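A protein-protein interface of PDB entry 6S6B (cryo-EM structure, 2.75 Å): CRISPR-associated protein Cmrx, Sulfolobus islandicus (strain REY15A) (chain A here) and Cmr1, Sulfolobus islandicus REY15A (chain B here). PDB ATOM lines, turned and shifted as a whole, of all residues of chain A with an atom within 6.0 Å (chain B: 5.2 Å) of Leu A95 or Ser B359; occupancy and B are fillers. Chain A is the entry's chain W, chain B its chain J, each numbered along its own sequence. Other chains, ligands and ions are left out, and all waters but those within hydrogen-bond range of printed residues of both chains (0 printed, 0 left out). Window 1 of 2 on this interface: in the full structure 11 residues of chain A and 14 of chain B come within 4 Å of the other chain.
Among the printed residues, pairs that only touch across the chains: Leu A95 with Ser B359, Arg A97 with Cys B355 and Lys A98 with Thr B362.
The side-chain amino group of Lys A98 sits close to the backbone carbonyl oxygen of Ser B359 (2.3 Å).
The backbone NH (N) of Arg A97 is in hydrogen-bond range of the side-chain hydroxyl (OG) of Ser B359 (3.0 Å).
Of the 14 printed residues of chain A, 3 touch a printed residue of chain B.
Along chain A the printed residues that touch a printed residue of chain B span positions 95 to 98.
Of the 8 printed residues of chain B, 3 touch a printed residue of chain A.
Among the printed residues, no Asp or Glu carboxylate lies within 4 Å of a Lys or Arg side-chain nitrogen of the other chain.
The backbone carbonyl oxygen (O) of Arg A97 lies within hydrogen-bond range of the backbone NH (N) of Asn A40, at 3.1 Å.
Val A43 touches none of the printed residues of chain B.
Of chain B, only Ser B359 comes within 4 Å of Leu A95.
Of the printed residues of chain B, Arg A97 touches Cys B355 (3.9 Å) and Ser B359 (3.0 Å).
Printed residues of chain B within 4 Å of Lys A98: Ser B359 (2.3 Å) and Thr B362 (3.5 Å).
Lys A99 touches none of the printed residues of chain B.
Ser B359 touches just these residues of chain A: Leu A95 (3.9 Å), Arg A97 (3.0 Å) and Lys A98 (2.3 Å).
The nearest printed residue of chain B that does not touch Leu A95 is Ile B360 (5.6 Å).
The nearest residue of chain A that does not touch Ser B359 is Ile A96 (4.02 Å).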
ATOM      1  N   ILE A  30      21.603  -1.777  15.239  1.00  0.00           N
ATOM      2  CA  ILE A  30      22.305  -0.564  15.644  1.00  0.00           C
ATOM      3  C   ILE A  30      22.941  -0.697  17.017  1.00  0.00           C
ATOM      4  O   ILE A  30      23.749   0.155  17.402  1.00  0.00           O
ATOM      5  CB  ILE A  30      21.354   0.650  15.639  1.00  0.00           C
ATOM      6  CG1 ILE A  30      22.124   1.955  15.416  1.00  0.00           C
ATOM      7  CG2 ILE A  30      20.600   0.727  16.945  1.00  0.00           C
ATOM      8  CD1 ILE A  30      22.549   2.199  13.996  1.00  0.00           C
ATOM      9  N   ASN A  40      24.048   1.377  22.840  1.00  0.00           N
ATOM     10  CA  ASN A  40      23.726   2.070  21.590  1.00  0.00           C
ATOM     11  C   ASN A  40      22.240   2.395  21.483  1.00  0.00           C
ATOM     12  O   ASN A  40      21.615   2.194  20.442  1.00  0.00           O
ATOM     13  CB  ASN A  40      24.189   1.259  20.382  1.00  0.00           C
ATOM     14  CG  ASN A  40      25.680   1.056  20.361  1.00  0.00           C
ATOM     15  OD1 ASN A  40      26.437   1.979  20.066  1.00  0.00           O
ATOM     16  ND2 ASN A  40      26.115  -0.154  20.686  1.00  0.00           N
ATOM     17  N   VAL A  41      21.671   2.903  22.558  1.00  0.00           N
ATOM     18  CA  VAL A  41      20.276   3.314  22.537  1.00  0.00           C
ATOM     19  C   VAL A  41      20.178   4.692  21.902  1.00  0.00           C
ATOM     20  O   VAL A  41      21.038   5.554  22.113  1.00  0.00           O
ATOM     21  CB  VAL A  41      19.693   3.297  23.959  1.00  0.00           C
ATOM     22  CG1 VAL A  41      19.717   1.887  24.507  1.00  0.00           C
ATOM     23  CG2 VAL A  41      20.469   4.229  24.868  1.00  0.00           C
ATOM     24  N   LEU A  42      19.134   4.908  21.114  1.00  0.00           N
ATOM     25  CA  LEU A  42      18.975   6.133  20.348  1.00  0.00           C
ATOM     26  C   LEU A  42      17.972   7.047  21.035  1.00  0.00           C
ATOM     27  O   LEU A  42      17.040   6.583  21.695  1.00  0.00           O
ATOM     28  CB  LEU A  42      18.530   5.820  18.916  1.00  0.00           C
ATOM     29  CG  LEU A  42      18.576   6.918  17.860  1.00  0.00           C
ATOM     30  CD1 LEU A  42      18.859   6.286  16.516  1.00  0.00           C
ATOM     31  CD2 LEU A  42      17.275   7.695  17.799  1.00  0.00           C
ATOM     32  N   VAL A  43      18.171   8.352  20.879  1.00  0.00           N
ATOM     33  CA  VAL A  43      17.364   9.357  21.558  1.00  0.00           C
ATOM     34  C   VAL A  43      16.872  10.374  20.541  1.00  0.00           C
ATOM     35  O   VAL A  43      17.659  10.893  19.742  1.00  0.00           O
ATOM     36  CB  VAL A  43      18.147  10.062  22.677  1.00  0.00           C
ATOM     37  CG1 VAL A  43      17.532  11.422  22.979  1.00  0.00           C
ATOM     38  CG2 VAL A  43      18.159   9.213  23.907  1.00  0.00           C
ATOM     39  N   LEU A  93      23.588  12.037  15.517  1.00  0.00           N
ATOM     40  CA  LEU A  93      22.675  11.095  16.154  1.00  0.00           C
ATOM     41  C   LEU A  93      23.092  10.920  17.607  1.00  0.00           C
ATOM     42  O   LEU A  93      24.125  10.302  17.888  1.00  0.00           O
ATOM     43  CB  LEU A  93      22.694   9.757  15.417  1.00  0.00           C
ATOM     44  CG  LEU A  93      21.529   8.794  15.602  1.00  0.00           C
ATOM     45  CD1 LEU A  93      20.270   9.387  15.008  1.00  0.00           C
ATOM     46  CD2 LEU A  93      21.861   7.465  14.946  1.00  0.00           C
ATOM     47  N   TYR A  94      22.293  11.454  18.528  1.00  0.00           N
ATOM     48  CA  TYR A  94      22.556  11.286  19.957  1.00  0.00           C
ATOM     49  C   TYR A  94      22.377   9.818  20.316  1.00  0.00           C
ATOM     50  O   TYR A  94      21.255   9.313  20.392  1.00  0.00           O
ATOM     51  CB  TYR A  94      21.633  12.172  20.787  1.00  0.00           C
ATOM     52  CG  TYR A  94      21.920  12.123  22.273  1.00  0.00           C
ATOM     53  CD1 TYR A  94      23.196  11.842  22.746  1.00  0.00           C
ATOM     54  CD2 TYR A  94      20.919  12.361  23.204  1.00  0.00           C
ATOM     55  CE1 TYR A  94      23.464  11.792  24.102  1.00  0.00           C
ATOM     56  CE2 TYR A  94      21.177  12.314  24.564  1.00  0.00           C
ATOM     57  CZ  TYR A  94      22.451  12.030  25.007  1.00  0.00           C
ATOM     58  OH  TYR A  94      22.719  11.983  26.357  1.00  0.00           O
ATOM     59  N   LEU A  95      23.492   9.129  20.541  1.00  0.00           N
ATOM     60  CA  LEU A  95      23.501   7.712  20.863  1.00  0.00           C
ATOM     61  C   LEU A  95      24.210   7.519  22.196  1.00  0.00           C
ATOM     62  O   LEU A  95      25.263   8.118  22.437  1.00  0.00           O
ATOM     63  CB  LEU A  95      24.208   6.908  19.767  1.00  0.00           C
ATOM     64  CG  LEU A  95      24.038   5.390  19.761  1.00  0.00           C
ATOM     65  CD1 LEU A  95      22.608   5.045  19.376  1.00  0.00           C
ATOM     66  CD2 LEU A  95      25.030   4.725  18.822  1.00  0.00           C
ATOM     67  N   ILE A  96      23.635   6.687  23.062  1.00  0.00           N
ATOM     68  CA  ILE A  96      24.138   6.478  24.415  1.00  0.00           C
ATOM     69  C   ILE A  96      24.705   5.071  24.522  1.00  0.00           C
ATOM     70  O   ILE A  96      24.118   4.116  24.002  1.00  0.00           O
ATOM     71  CB  ILE A  96      23.038   6.712  25.473  1.00  0.00           C
ATOM     72  CG1 ILE A  96      22.685   8.199  25.556  1.00  0.00           C
ATOM     73  CG2 ILE A  96      23.460   6.172  26.830  1.00  0.00           C
ATOM     74  CD1 ILE A  96      21.599   8.628  24.612  1.00  0.00           C
ATOM     75  N   ARG A  97      25.844   4.951  25.212  1.00  0.00           N
ATOM     76  CA  ARG A  97      26.607   3.705  25.300  1.00  0.00           C
ATOM     77  C   ARG A  97      27.093   3.275  23.919  1.00  0.00           C
ATOM     78  O   ARG A  97      26.952   2.120  23.513  1.00  0.00           O
ATOM     79  CB  ARG A  97      25.801   2.591  25.971  1.00  0.00           C
ATOM     80  CG  ARG A  97      25.227   2.954  27.324  1.00  0.00           C
ATOM     81  CD  ARG A  97      24.310   1.851  27.830  1.00  0.00           C
ATOM     82  NE  ARG A  97      24.050   1.967  29.261  1.00  0.00           N
ATOM     83  CZ  ARG A  97      24.846   1.489  30.208  1.00  0.00           C
ATOM     84  NH1 ARG A  97      25.963   0.852  29.884  1.00  0.00           N
ATOM     85  NH2 ARG A  97      24.524   1.645  31.484  1.00  0.00           N
ATOM     86  N   LYS A  98      27.669   4.227  23.192  1.00  0.00           N
ATOM     87  CA  LYS A  98      28.212   3.936  21.875  1.00  0.00           C
ATOM     88  C   LYS A  98      29.390   2.981  21.990  1.00  0.00           C
ATOM     89  O   LYS A  98      30.358   3.251  22.707  1.00  0.00           O
ATOM     90  CB  LYS A  98      28.649   5.226  21.187  1.00  0.00           C
ATOM     91  CG  LYS A  98      27.623   6.339  21.236  1.00  0.00           C
ATOM     92  CD  LYS A  98      27.753   7.260  20.034  1.00  0.00           C
ATOM     93  CE  LYS A  98      29.208   7.529  19.683  1.00  0.00           C
ATOM     94  NZ  LYS A  98      29.941   8.212  20.784  1.00  0.00           N
ATOM     95  N   LYS A  99      29.304   1.856  21.282  1.00  0.00           N
ATOM     96  CA  LYS A  99      30.359   0.855  21.288  1.00  0.00           C
ATOM     97  C   LYS A  99      30.968   0.620  19.917  1.00  0.00           C
ATOM     98  O   LYS A  99      31.931  -0.149  19.810  1.00  0.00           O
ATOM     99  CB  LYS A  99      29.834  -0.475  21.844  1.00  0.00           C
ATOM    100  CG  LYS A  99      29.125  -0.360  23.184  1.00  0.00           C
ATOM    101  CD  LYS A  99      29.951   0.414  24.204  1.00  0.00           C
ATOM    102  CE  LYS A  99      31.253  -0.291  24.532  1.00  0.00           C
ATOM    103  NZ  LYS A  99      31.039  -1.741  24.773  1.00  0.00           N
ATOM    104  N   GLY A 100      30.447   1.253  18.869  1.00  0.00           N
ATOM    105  CA  GLY A 100      30.987   1.071  17.540  1.00  0.00           C
ATOM    106  C   GLY A 100      31.076   2.391  16.801  1.00  0.00           C
ATOM    107  O   GLY A 100      30.336   3.338  17.076  1.00  0.00           O
ATOM    108  N   ILE A 102      30.368   4.286  13.529  1.00  0.00           N
ATOM    109  CA  ILE A 102      29.383   4.162  12.465  1.00  0.00           C
ATOM    110  C   ILE A 102      29.696   5.241  11.437  1.00  0.00           C
ATOM    111  O   ILE A 102      29.202   6.369  11.530  1.00  0.00           O
ATOM    112  CB  ILE A 102      27.952   4.287  12.998  1.00  0.00           C
ATOM    113  CG1 ILE A 102      27.798   3.500  14.302  1.00  0.00           C
ATOM    114  CG2 ILE A 102      26.968   3.782  11.972  1.00  0.00           C
ATOM    115  CD1 ILE A 102      27.726   2.003  14.111  1.00  0.00           C
ATOM    116  N   CYS B 355      29.709   6.179  31.844  1.00  0.00           N
ATOM    117  CA  CYS B 355      28.947   5.962  30.622  1.00  0.00           C
ATOM    118  C   CYS B 355      28.107   7.171  30.231  1.00  0.00           C
ATOM    119  O   CYS B 355      26.917   7.034  29.929  1.00  0.00           O
ATOM    120  CB  CYS B 355      28.040   4.739  30.779  1.00  0.00           C
ATOM    121  SG  CYS B 355      28.913   3.174  30.994  1.00  0.00           S
ATOM    122  N   CYS B 356      28.708   8.354  30.236  1.00  0.00           N
ATOM    123  CA  CYS B 356      28.134   9.505  29.546  1.00  0.00           C
ATOM    124  C   CYS B 356      29.113  10.282  28.685  1.00  0.00           C
ATOM    125  O   CYS B 356      28.686  10.849  27.675  1.00  0.00           O
ATOM    126  CB  CYS B 356      27.469  10.465  30.529  1.00  0.00           C
ATOM    127  SG  CYS B 356      25.764  10.053  30.847  1.00  0.00           S
ATOM    128  N   ILE B 357      30.398  10.339  29.021  1.00  0.00           N
ATOM    129  CA  ILE B 357      31.373  10.983  28.155  1.00  0.00           C
ATOM    130  C   ILE B 357      32.229   9.982  27.415  1.00  0.00           C
ATOM    131  O   ILE B 357      33.011  10.380  26.542  1.00  0.00           O
ATOM    132  CB  ILE B 357      32.255  11.978  28.927  1.00  0.00           C
ATOM    133  CG1 ILE B 357      32.897  11.309  30.133  1.00  0.00           C
ATOM    134  CG2 ILE B 357      31.441  13.178  29.352  1.00  0.00           C
ATOM    135  CD1 ILE B 357      34.013  12.129  30.712  1.00  0.00           C
ATOM    136  N   LYS B 358      32.116   8.693  27.729  1.00  0.00           N
ATOM    137  CA  LYS B 358      32.624   7.673  26.824  1.00  0.00           C
ATOM    138  C   LYS B 358      31.739   7.521  25.601  1.00  0.00           C
ATOM    139  O   LYS B 358      32.047   6.724  24.710  1.00  0.00           O
ATOM    140  CB  LYS B 358      32.764   6.331  27.549  1.00  0.00           C
ATOM    141  CG  LYS B 358      31.463   5.756  28.059  1.00  0.00           C
ATOM    142  CD  LYS B 358      31.697   4.443  28.786  1.00  0.00           C
ATOM    143  CE  LYS B 358      31.775   3.276  27.816  1.00  0.00           C
ATOM    144  NZ  LYS B 358      31.691   1.966  28.513  1.00  0.00           N
ATOM    145  N   SER B 359      30.642   8.276  25.557  1.00  0.00           N
ATOM    146  CA  SER B 359      29.770   8.347  24.394  1.00  0.00           C
ATOM    147  C   SER B 359      29.907   9.683  23.679  1.00  0.00           C
ATOM    148  O   SER B 359      30.096   9.706  22.460  1.00  0.00           O
ATOM    149  CB  SER B 359      28.314   8.109  24.819  1.00  0.00           C
ATOM    150  OG  SER B 359      28.173   6.865  25.480  1.00  0.00           O
ATOM    151  N   ILE B 360      29.815  10.800  24.402  1.00  0.00           N
ATOM    152  CA  ILE B 360      29.842  12.120  23.785  1.00  0.00           C
ATOM    153  C   ILE B 360      31.215  12.390  23.196  1.00  0.00           C
ATOM    154  O   ILE B 360      31.364  12.543  21.978  1.00  0.00           O
ATOM    155  CB  ILE B 360      29.466  13.208  24.803  1.00  0.00           C
ATOM    156  CG1 ILE B 360      28.037  13.003  25.295  1.00  0.00           C
ATOM    157  CG2 ILE B 360      29.632  14.586  24.194  1.00  0.00           C
ATOM    158  CD1 ILE B 360      27.748  13.700  26.599  1.00  0.00           C
ATOM    159  N   ILE B 361      32.231  12.444  24.051  1.00  0.00           N
ATOM    160  CA  ILE B 361      33.615  12.628  23.592  1.00  0.00           C
ATOM    161  C   ILE B 361      34.225  11.233  23.542  1.00  0.00           C
ATOM    162  O   ILE B 361      34.836  10.739  24.490  1.00  0.00           O
ATOM    163  CB  ILE B 361      34.392  13.600  24.481  1.00  0.00           C
ATOM    164  CG1 ILE B 361      33.967  13.429  25.938  1.00  0.00           C
ATOM    165  CG2 ILE B 361      34.181  15.031  24.021  1.00  0.00           C
ATOM    166  CD1 ILE B 361      34.640  14.386  26.889  1.00  0.00           C
ATOM    167  N   THR B 362      34.060  10.586  22.394  1.00  0.00           N
ATOM    168  CA  THR B 362      34.379   9.173  22.280  1.00  0.00           C
ATOM    169  C   THR B 362      35.828   8.947  21.859  1.00  0.00           C
ATOM    170  O   THR B 362      36.123   8.526  20.738  1.00  0.00           O
ATOM    171  CB  THR B 362      33.416   8.499  21.299  1.00  0.00           C
ATOM    172  OG1 THR B 362      33.813   7.138  21.081  1.00  0.00           O
ATOM    173  CG2 THR B 362      33.324   9.266  19.983  1.00  0.00           C
